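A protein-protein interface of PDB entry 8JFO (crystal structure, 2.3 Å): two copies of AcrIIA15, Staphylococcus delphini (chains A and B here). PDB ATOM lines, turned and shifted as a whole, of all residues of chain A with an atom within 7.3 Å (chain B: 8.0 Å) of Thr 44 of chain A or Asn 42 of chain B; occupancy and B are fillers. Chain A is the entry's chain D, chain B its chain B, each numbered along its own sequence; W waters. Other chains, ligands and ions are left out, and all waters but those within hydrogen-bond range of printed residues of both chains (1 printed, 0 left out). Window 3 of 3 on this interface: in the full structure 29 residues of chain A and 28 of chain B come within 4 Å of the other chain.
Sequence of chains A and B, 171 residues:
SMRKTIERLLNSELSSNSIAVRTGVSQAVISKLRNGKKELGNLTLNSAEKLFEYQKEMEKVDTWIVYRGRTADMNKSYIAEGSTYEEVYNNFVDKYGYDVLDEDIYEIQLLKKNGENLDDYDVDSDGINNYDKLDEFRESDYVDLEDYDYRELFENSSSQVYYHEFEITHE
Water W1 bridges OE2 of Glu 49 of chain A (2.7 Å) and N of Arg 3 of chain B (3.4 Å).
Of the 15 printed residues of chain B, 8 touch a printed residue of chain A.
Hydrophobic or aromatic side chains of chain B within 4 Å of the printed part of chain A: Leu 45.
Of the 15 printed residues of chain A, 9 touch a printed residue of chain B.
Printed residues of chain A that touch a printed residue of chain B: Ser 1, Leu 40, Gly 41, Asn 42, Leu 43, Thr 44, Leu 45, Asn 46 and Glu 49.
Hydrophobic or aromatic side chains of chain A that line the printed part of chain B: Leu 45.
Along chain A the printed residues that touch a printed residue of chain B span positions 1 to 49.
Among the printed residues, 18 pairs touch across the chains.
Among the printed residues, Asp or Glu carboxylates within 4 Å of a Lys or Arg side-chain nitrogen of the other chain: Glu 49 of chain A with Arg 3 of chain B (2.9 Å).
Gly 41 of chain A touches Leu 45 of chain B, and with the chains exchanged Leu 45 of chain A touches Gly 41 of chain B.
Leu 43 of chain A touches Thr 44 of chain B, and with the chains exchanged Thr 44 of chain A touches Leu 43 of chain B.
Leu 43 of chain A touches Leu 45 of chain B, and with the chains exchanged Leu 45 of chain A touches Leu 43 of chain B.
Thr 44 of chain A touches Asn 42 of chain B, but with the chains exchanged Asn 42 of chain A does not touch Thr 44 of chain B (4.1 Å).
Positions printed for both chains: 29, 38, 40, 41, 42, 43, 44, 45, 46, 47 and 48.
Of the 18 pairs that touch across the chains among the printed residues, 14 have their exchanged pair printed and touching as well.
NE of Arg 3 of chain B is in salt-bridge range of OE2 of Glu 49 of chain A, at 2.9 Å.
N of Leu 45 of chain B sits at hydrogen-bond distance from O of Gly 41 of chain A, at 3.2 Å.
NH2 of Arg 3 of chain B sits at hydrogen-bond distance from OD1 of Asn 46 of chain A (2.6 Å).
The backbone carbonyl oxygen (O) of Gly 41 of chain B sits at hydrogen-bond distance from the backbone NH (N) of Asn 46 of chain A (3.1 Å).
The backbone NH (N) of Leu 45 of chain B sits at hydrogen-bond distance from the backbone carbonyl oxygen (O) of Leu 43 of chain A, 2.8 Å away.
The backbone carbonyl oxygen (O) of Gly 41 of chain A sits at hydrogen-bond distance from the backbone NH (N) of Asn 46 of chain B.
The backbone NH of Leu 45 of chain A lies within hydrogen-bond range of the backbone carbonyl oxygen of Gly 41 of chain B (2.9 Å).
The backbone carbonyl oxygen (O) of Leu 43 of chain B lies within hydrogen-bond range of the backbone NH (N) of Leu 45 of chain A.
The side-chain hydroxyl (OG) of Ser 47 of chain A sits at hydrogen-bond distance from the side-chain hydroxyl (OG1) of Thr 44 of chain A (3.2 Å).
The backbone NH (N) of Ser 47 of chain B is in hydrogen-bond range of the side-chain hydroxyl (OG1) of Thr 44 of chain B.
NZ of Lys 38 of chain A lies within hydrogen-bond range of OD1 of Asn 42 of chain A (2.9 Å).
The side-chain amino group (NZ) of Lys 38 of chain B sits at hydrogen-bond distance from the backbone carbonyl oxygen (O) of Asn 42 of chain B.
Ser 1 of chain A touches Leu 45 of chain B (O to CD1, 3.7 Å).
CD2 of Leu 45 of chain B touches O of Leu 40 of chain A (3.8 Å).
Thr 44 of chain B touches Gly 41 of chain A.
N of Asn 42 of chain A touches ND2 of Asn 46 of chain B, at 3.9 Å.
O of Leu 43 of chain A touches CA of Thr 44 of chain B, 3.5 Å away.
Thr 44 of chain A touches Gly 41 of chain B (CB to O, 3.4 Å).
Asn 42 of chain B touches Thr 44 of chain A.
Thr 44 of chain A touches Leu 43 of chain B.
O of Leu 40 of chain B touches CD2 of Leu 45 of chain A, at 3.6 Å.
Asn 46 of chain A touches Asn 42 of chain B.
Thr 44 of chain A touches just these residues of chain B: Gly 41 (3.4 Å), Asn 42 (3.8 Å) and Leu 43 (3.6 Å).
Printed residues of chain B within 4 Å of Leu 45 of chain A: Leu 40 (3.6 Å), Gly 41 (2.9 Å) and Leu 43 (2.9 Å).
Lys 37 of chain B touches none of the printed residues of chain A.
Printed residues of chain A within 4 Å of Leu 40 of chain B: Leu 45 (3.6 Å).
Gly 41 of chain B touches three residues of chain A.
Of chain A, only Thr 44 and Asn 46 come within 4 Å of Asn 42 of chain B.
The nearest residue of chain B that does not touch Thr 44 of chain A is Thr 44 of chain B (4.4 Å).
The nearest residue of chain A that does not touch Asn 42 of chain B is Leu 45 of chain A (4.8 Å).
The nearest printed residue of chain B that does not touch Asn 46 of chain A is Glu 39 of chain B (5.3 Å).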
ATOM      1  N   SER A   1       5.660  -9.379   7.386  1.00  0.00           N
ATOM      2  CA  SER A   1       4.957 -10.530   6.772  1.00  0.00           C
ATOM      3  C   SER A   1       5.756 -11.809   7.035  1.00  0.00           C
ATOM      4  O   SER A   1       6.885 -11.894   6.526  1.00  0.00           O
ATOM      5  CB  SER A   1       4.822 -10.261   5.333  1.00  0.00           C
ATOM      6  N   ILE A   6       4.620 -16.937   3.386  1.00  0.00           N
ATOM      7  CA  ILE A   6       5.093 -16.608   2.008  1.00  0.00           C
ATOM      8  C   ILE A   6       5.657 -17.881   1.362  1.00  0.00           C
ATOM      9  O   ILE A   6       5.377 -18.109   0.184  1.00  0.00           O
ATOM     10  CB  ILE A   6       6.087 -15.433   2.025  1.00  0.00           C
ATOM     11  CG1 ILE A   6       5.499 -14.213   2.736  1.00  0.00           C
ATOM     12  CG2 ILE A   6       6.543 -15.093   0.617  1.00  0.00           C
ATOM     13  CD1 ILE A   6       6.496 -13.110   2.981  1.00  0.00           C
ATOM     14  N   VAL A  29      10.381 -11.081  -9.818  1.00  0.00           N
ATOM     15  CA  VAL A  29      10.712 -11.268  -8.380  1.00  0.00           C
ATOM     16  C   VAL A  29      10.263 -12.669  -7.954  1.00  0.00           C
ATOM     17  O   VAL A  29      11.071 -13.366  -7.332  1.00  0.00           O
ATOM     18  CB  VAL A  29      10.098 -10.157  -7.509  1.00  0.00           C
ATOM     19  CG1 VAL A  29       9.962 -10.587  -6.061  1.00  0.00           C
ATOM     20  CG2 VAL A  29      10.886  -8.862  -7.612  1.00  0.00           C
ATOM     21  N   LYS A  38      16.994 -15.021  -5.790  1.00  0.00           N
ATOM     22  CA  LYS A  38      16.739 -13.961  -4.782  1.00  0.00           C
ATOM     23  C   LYS A  38      16.242 -14.633  -3.502  1.00  0.00           C
ATOM     24  O   LYS A  38      15.273 -15.394  -3.583  1.00  0.00           O
ATOM     25  CB  LYS A  38      15.704 -12.955  -5.291  1.00  0.00           C
ATOM     26  CG  LYS A  38      15.383 -11.796  -4.360  1.00  0.00           C
ATOM     27  CD  LYS A  38      14.165 -11.026  -4.811  1.00  0.00           C
ATOM     28  CE  LYS A  38      13.948  -9.743  -4.041  1.00  0.00           C
ATOM     29  NZ  LYS A  38      14.977  -8.731  -4.367  1.00  0.00           N
ATOM     30  N   LEU A  40      14.319 -14.898   0.120  1.00  0.00           N
ATOM     31  CA  LEU A  40      13.049 -14.308   0.612  1.00  0.00           C
ATOM     32  C   LEU A  40      13.346 -13.119   1.533  1.00  0.00           C
ATOM     33  O   LEU A  40      12.578 -12.148   1.502  1.00  0.00           O
ATOM     34  CB  LEU A  40      12.261 -15.406   1.332  1.00  0.00           C
ATOM     35  CG  LEU A  40      10.867 -15.025   1.826  1.00  0.00           C
ATOM     36  CD1 LEU A  40      10.060 -14.381   0.712  1.00  0.00           C
ATOM     37  CD2 LEU A  40      10.143 -16.244   2.371  1.00  0.00           C
ATOM     38  N   GLY A  41      14.425 -13.199   2.313  1.00  0.00           N
ATOM     39  CA  GLY A  41      14.746 -12.098   3.201  1.00  0.00           C
ATOM     40  C   GLY A  41      15.108 -10.816   2.478  1.00  0.00           C
ATOM     41  O   GLY A  41      15.043  -9.735   3.080  1.00  0.00           O
ATOM     42  N   ASN A  42      15.482 -10.909   1.196  1.00  0.00           N
ATOM     43  CA  ASN A  42      15.843  -9.745   0.391  1.00  0.00           C
ATOM     44  C   ASN A  42      14.637  -9.026  -0.189  1.00  0.00           C
ATOM     45  O   ASN A  42      14.785  -7.923  -0.722  1.00  0.00           O
ATOM     46  CB  ASN A  42      16.777 -10.156  -0.766  1.00  0.00           C
ATOM     47  CG  ASN A  42      17.373  -8.954  -1.494  1.00  0.00           C
ATOM     48  OD1 ASN A  42      17.297  -8.865  -2.716  1.00  0.00           O
ATOM     49  ND2 ASN A  42      17.945  -8.020  -0.742  1.00  0.00           N
ATOM     50  N   LEU A  43      13.455  -9.622  -0.107  1.00  0.00           N
ATOM     51  CA  LEU A  43      12.236  -8.934  -0.505  1.00  0.00           C
ATOM     52  C   LEU A  43      12.019  -7.686   0.343  1.00  0.00           C
ATOM     53  O   LEU A  43      12.318  -7.670   1.541  1.00  0.00           O
ATOM     54  CB  LEU A  43      11.054  -9.882  -0.352  1.00  0.00           C
ATOM     55  CG  LEU A  43       9.865  -9.875  -1.302  1.00  0.00           C
ATOM     56  CD1 LEU A  43      10.287  -9.675  -2.744  1.00  0.00           C
ATOM     57  CD2 LEU A  43       9.137 -11.189  -1.126  1.00  0.00           C
ATOM     58  N   THR A  44      11.509  -6.630  -0.280  1.00  0.00           N
ATOM     59  CA  THR A  44      11.117  -5.465   0.500  1.00  0.00           C
ATOM     60  C   THR A  44       9.904  -5.799   1.367  1.00  0.00           C
ATOM     61  O   THR A  44       9.176  -6.768   1.127  1.00  0.00           O
ATOM     62  CB  THR A  44      10.746  -4.281  -0.391  1.00  0.00           C
ATOM     63  OG1 THR A  44       9.638  -4.651  -1.226  1.00  0.00           O
ATOM     64  CG2 THR A  44      11.922  -3.847  -1.247  1.00  0.00           C
ATOM     65  N   LEU A  45       9.691  -4.969   2.389  1.00  0.00           N
ATOM     66  CA  LEU A  45       8.563  -5.167   3.290  1.00  0.00           C
ATOM     67  C   LEU A  45       7.231  -5.046   2.563  1.00  0.00           C
ATOM     68  O   LEU A  45       6.315  -5.837   2.819  1.00  0.00           O
ATOM     69  CB  LEU A  45       8.635  -4.164   4.438  1.00  0.00           C
ATOM     70  CG  LEU A  45       7.730  -4.482   5.626  1.00  0.00           C
ATOM     71  CD1 LEU A  45       8.041  -5.867   6.171  1.00  0.00           C
ATOM     72  CD2 LEU A  45       7.887  -3.423   6.702  1.00  0.00           C
ATOM     73  N   ASN A  46       7.106  -4.083   1.638  1.00  0.00           N
ATOM     74  CA  ASN A  46       5.860  -3.916   0.882  1.00  0.00           C
ATOM     75  C   ASN A  46       5.482  -5.185   0.119  1.00  0.00           C
ATOM     76  O   ASN A  46       4.347  -5.677   0.219  1.00  0.00           O
ATOM     77  CB  ASN A  46       5.979  -2.752  -0.100  1.00  0.00           C
ATOM     78  CG  ASN A  46       5.971  -1.405   0.578  1.00  0.00           C
ATOM     79  OD1 ASN A  46       5.172  -1.152   1.481  1.00  0.00           O
ATOM     80  ND2 ASN A  46       6.828  -0.504   0.106  1.00  0.00           N
ATOM     81  N   SER A  47       6.426  -5.726  -0.663  1.00  0.00           N
ATOM     82  CA  SER A  47       6.137  -6.915  -1.468  1.00  0.00           C
ATOM     83  C   SER A  47       5.893  -8.127  -0.579  1.00  0.00           C
ATOM     84  O   SER A  47       5.057  -8.988  -0.898  1.00  0.00           O
ATOM     85  CB  SER A  47       7.290  -7.201  -2.432  1.00  0.00           C
ATOM     86  OG  SER A  47       7.572  -6.090  -3.259  1.00  0.00           O
ATOM     87  N   ALA A  48       6.640  -8.225   0.527  1.00  0.00           N
ATOM     88  CA  ALA A  48       6.416  -9.313   1.466  1.00  0.00           C
ATOM     89  C   ALA A  48       5.004  -9.257   2.025  1.00  0.00           C
ATOM     90  O   ALA A  48       4.329 -10.287   2.128  1.00  0.00           O
ATOM     91  CB  ALA A  48       7.440  -9.262   2.597  1.00  0.00           C
ATOM     92  N   GLU A  49       4.535  -8.059   2.374  1.00  0.00           N
ATOM     93  CA  GLU A  49       3.166  -7.907   2.852  1.00  0.00           C
ATOM     94  C   GLU A  49       2.160  -8.324   1.792  1.00  0.00           C
ATOM     95  O   GLU A  49       1.165  -8.986   2.101  1.00  0.00           O
ATOM     96  CB  GLU A  49       2.911  -6.468   3.296  1.00  0.00           C
ATOM     97  CG  GLU A  49       3.547  -6.122   4.627  1.00  0.00           C
ATOM     98  CD  GLU A  49       3.591  -4.626   4.878  1.00  0.00           C
ATOM     99  OE1 GLU A  49       3.350  -3.847   3.922  1.00  0.00           O
ATOM    100  OE2 GLU A  49       3.866  -4.232   6.037  1.00  0.00           O
ATOM    101  N   LYS A  50       2.383  -7.931   0.539  1.00  0.00           N
ATOM    102  CA  LYS A  50       1.422  -8.309  -0.498  1.00  0.00           C
ATOM    103  C   LYS A  50       1.324  -9.828  -0.624  1.00  0.00           C
ATOM    104  O   LYS A  50       0.220 -10.395  -0.650  1.00  0.00           O
ATOM    105  CB  LYS A  50       1.796  -7.665  -1.827  1.00  0.00           C
ATOM    106  CG  LYS A  50       1.863  -6.153  -1.749  1.00  0.00           C
ATOM    107  CD  LYS A  50       2.042  -5.541  -3.130  1.00  0.00           C
ATOM    108  CE  LYS A  50       1.923  -4.033  -3.066  1.00  0.00           C
ATOM    109  NZ  LYS A  50       3.004  -3.355  -3.838  1.00  0.00           N
ATOM    110  N   ARG B   3       4.800  -3.544  10.850  1.00  0.00           N
ATOM    111  CA  ARG B   3       5.171  -2.121  10.807  1.00  0.00           C
ATOM    112  C   ARG B   3       4.945  -1.488  12.166  1.00  0.00           C
ATOM    113  O   ARG B   3       5.907  -0.956  12.692  1.00  0.00           O
ATOM    114  CB  ARG B   3       4.273  -1.421   9.789  1.00  0.00           C
ATOM    115  CG  ARG B   3       4.615  -1.719   8.345  1.00  0.00           C
ATOM    116  CD  ARG B   3       3.714  -0.851   7.503  1.00  0.00           C
ATOM    117  NE  ARG B   3       3.841  -1.290   6.132  1.00  0.00           N
ATOM    118  CZ  ARG B   3       4.649  -0.739   5.245  1.00  0.00           C
ATOM    119  NH1 ARG B   3       5.392   0.303   5.570  1.00  0.00           N
ATOM    120  NH2 ARG B   3       4.695  -1.230   4.028  1.00  0.00           N
ATOM    121  N   VAL B  29      20.628   3.067   7.909  1.00  0.00           N
ATOM    122  CA  VAL B  29      19.237   2.712   7.621  1.00  0.00           C
ATOM    123  C   VAL B  29      18.287   3.263   8.687  1.00  0.00           C
ATOM    124  O   VAL B  29      17.234   3.812   8.358  1.00  0.00           O
ATOM    125  CB  VAL B  29      19.093   1.188   7.470  1.00  0.00           C
ATOM    126  CG1 VAL B  29      17.840   0.853   6.657  1.00  0.00           C
ATOM    127  CG2 VAL B  29      20.347   0.602   6.835  1.00  0.00           C
ATOM    128  N   LEU B  33      15.288   5.979   7.910  1.00  0.00           N
ATOM    129  CA  LEU B  33      13.866   5.711   8.252  1.00  0.00           C
ATOM    130  C   LEU B  33      13.331   6.895   9.059  1.00  0.00           C
ATOM    131  O   LEU B  33      12.236   7.381   8.732  1.00  0.00           O
ATOM    132  CB  LEU B  33      13.773   4.409   9.052  1.00  0.00           C
ATOM    133  CG  LEU B  33      14.100   3.131   8.281  1.00  0.00           C
ATOM    134  CD1 LEU B  33      14.288   1.957   9.228  1.00  0.00           C
ATOM    135  CD2 LEU B  33      13.027   2.822   7.254  1.00  0.00           C
ATOM    136  N   LYS B  37      14.158   9.579   4.522  1.00  0.00           N
ATOM    137  CA  LYS B  37      14.921   9.258   3.288  1.00  0.00           C
ATOM    138  C   LYS B  37      14.549   7.842   2.839  1.00  0.00           C
ATOM    139  O   LYS B  37      14.403   7.628   1.622  1.00  0.00           O
ATOM    140  CB  LYS B  37      16.427   9.365   3.539  1.00  0.00           C
ATOM    141  N   LYS B  38      14.391   6.921   3.794  1.00  0.00           N
ATOM    142  CA  LYS B  38      13.981   5.564   3.452  1.00  0.00           C
ATOM    143  C   LYS B  38      12.604   5.275   4.038  1.00  0.00           C
ATOM    144  O   LYS B  38      12.384   5.451   5.243  1.00  0.00           O
ATOM    145  CB  LYS B  38      14.996   4.534   3.959  1.00  0.00           C
ATOM    146  CG  LYS B  38      14.838   3.136   3.351  1.00  0.00           C
ATOM    147  CD  LYS B  38      15.936   2.200   3.860  1.00  0.00           C
ATOM    148  CE  LYS B  38      15.811   0.784   3.290  1.00  0.00           C
ATOM    149  NZ  LYS B  38      15.898   0.739   1.800  1.00  0.00           N
ATOM    150  N   GLU B  39      11.684   4.837   3.186  1.00  0.00           N
ATOM    151  CA  GLU B  39      10.379   4.411   3.661  1.00  0.00           C
ATOM    152  C   GLU B  39      10.466   3.016   4.266  1.00  0.00           C
ATOM    153  O   GLU B  39      11.278   2.182   3.852  1.00  0.00           O
ATOM    154  CB  GLU B  39       9.361   4.423   2.527  1.00  0.00           C
ATOM    155  CG  GLU B  39       9.230   5.768   1.866  1.00  0.00           C
ATOM    156  CD  GLU B  39       8.167   5.777   0.797  1.00  0.00           C
ATOM    157  OE1 GLU B  39       7.481   4.746   0.638  1.00  0.00           O
ATOM    158  OE2 GLU B  39       8.013   6.813   0.114  1.00  0.00           O
ATOM    159  N   LEU B  40       9.648   2.747   5.289  1.00  0.00           N
ATOM    160  CA  LEU B  40       9.688   1.436   6.001  1.00  0.00           C
ATOM    161  C   LEU B  40       9.397   0.286   5.032  1.00  0.00           C
ATOM    162  O   LEU B  40       9.947  -0.803   5.233  1.00  0.00           O
ATOM    163  CB  LEU B  40       8.673   1.468   7.148  1.00  0.00           C
ATOM    164  CG  LEU B  40       8.804   0.352   8.181  1.00  0.00           C
ATOM    165  CD1 LEU B  40      10.226   0.274   8.710  1.00  0.00           C
ATOM    166  CD2 LEU B  40       7.824   0.561   9.322  1.00  0.00           C
ATOM    167  N   GLY B  41       8.569   0.527   4.020  1.00  0.00           N
ATOM    168  CA  GLY B  41       8.228  -0.508   3.026  1.00  0.00           C
ATOM    169  C   GLY B  41       9.437  -0.967   2.236  1.00  0.00           C
ATOM    170  O   GLY B  41       9.464  -2.139   1.847  1.00  0.00           O
ATOM    171  N   ASN B  42      10.360  -0.053   1.937  1.00  0.00           N
ATOM    172  CA  ASN B  42      11.588  -0.379   1.163  1.00  0.00           C
ATOM    173  C   ASN B  42      12.601  -1.147   2.022  1.00  0.00           C
ATOM    174  O   ASN B  42      13.539  -1.713   1.445  1.00  0.00           O
ATOM    175  CB  ASN B  42      12.164   0.868   0.493  1.00  0.00           C
ATOM    176  CG  ASN B  42      11.162   1.541  -0.419  1.00  0.00           C
ATOM    177  OD1 ASN B  42      10.331   0.875  -1.034  1.00  0.00           O
ATOM    178  ND2 ASN B  42      11.231   2.859  -0.516  1.00  0.00           N
ATOM    179  N   LEU B  43      12.423  -1.159   3.343  1.00  0.00           N
ATOM    180  CA  LEU B  43      13.324  -1.945   4.223  1.00  0.00           C
ATOM    181  C   LEU B  43      13.201  -3.423   3.856  1.00  0.00           C
ATOM    182  O   LEU B  43      12.080  -3.881   3.599  1.00  0.00           O
ATOM    183  CB  LEU B  43      12.934  -1.704   5.682  1.00  0.00           C
ATOM    184  CG  LEU B  43      13.904  -2.214   6.744  1.00  0.00           C
ATOM    185  CD1 LEU B  43      15.260  -1.557   6.584  1.00  0.00           C
ATOM    186  CD2 LEU B  43      13.357  -1.939   8.133  1.00  0.00           C
ATOM    187  N   THR B  44      14.326  -4.127   3.824  1.00  0.00           N
ATOM    188  CA  THR B  44      14.315  -5.560   3.456  1.00  0.00           C
ATOM    189  C   THR B  44      13.636  -6.344   4.573  1.00  0.00           C
ATOM    190  O   THR B  44      13.638  -5.864   5.717  1.00  0.00           O
ATOM    191  CB  THR B  44      15.728  -6.103   3.214  1.00  0.00           C
ATOM    192  OG1 THR B  44      16.489  -5.924   4.408  1.00  0.00           O
ATOM    193  CG2 THR B  44      16.425  -5.452   2.040  1.00  0.00           C
ATOM    194  N   LEU B  45      13.089  -7.507   4.238  1.00  0.00           N
ATOM    195  CA  LEU B  45      12.481  -8.352   5.253  1.00  0.00           C
ATOM    196  C   LEU B  45      13.490  -8.714   6.335  1.00  0.00           C
ATOM    197  O   LEU B  45      13.145  -8.755   7.520  1.00  0.00           O
ATOM    198  CB  LEU B  45      11.894  -9.610   4.611  1.00  0.00           C
ATOM    199  CG  LEU B  45      11.064 -10.528   5.509  1.00  0.00           C
ATOM    200  CD1 LEU B  45       9.881  -9.763   6.093  1.00  0.00           C
ATOM    201  CD2 LEU B  45      10.592 -11.766   4.754  1.00  0.00           C
ATOM    202  N   ASN B  46      14.746  -8.961   5.958  1.00  0.00           N
ATOM    203  CA  ASN B  46      15.758  -9.296   6.962  1.00  0.00           C
ATOM    204  C   ASN B  46      15.871  -8.207   8.033  1.00  0.00           C
ATOM    205  O   ASN B  46      15.771  -8.482   9.240  1.00  0.00           O
ATOM    206  CB  ASN B  46      17.106  -9.518   6.278  1.00  0.00           C
ATOM    207  CG  ASN B  46      17.188 -10.856   5.560  1.00  0.00           C
ATOM    208  OD1 ASN B  46      16.740 -11.873   6.083  1.00  0.00           O
ATOM    209  ND2 ASN B  46      17.767 -10.860   4.356  1.00  0.00           N
ATOM    210  N   SER B  47      16.052  -6.956   7.609  1.00  0.00           N
ATOM    211  CA  SER B  47      16.265  -5.878   8.572  1.00  0.00           C
ATOM    212  C   SER B  47      14.993  -5.552   9.348  1.00  0.00           C
ATOM    213  O   SER B  47      15.040  -5.299  10.566  1.00  0.00           O
ATOM    214  CB  SER B  47      16.810  -4.646   7.852  1.00  0.00           C
ATOM    215  OG  SER B  47      18.080  -4.947   7.299  1.00  0.00           O
ATOM    216  N   ALA B  48      13.851  -5.588   8.663  1.00  0.00           N
ATOM    217  CA  ALA B  48      12.560  -5.352   9.344  1.00  0.00           C
ATOM    218  C   ALA B  48      12.379  -6.379  10.466  1.00  0.00           C
ATOM    219  O   ALA B  48      11.980  -5.984  11.561  1.00  0.00           O
ATOM    220  CB  ALA B  48      11.434  -5.404   8.352  1.00  0.00           C
HETATM  221  O   HOH W   1       4.104  -5.645   8.335  1.00  0.00           O
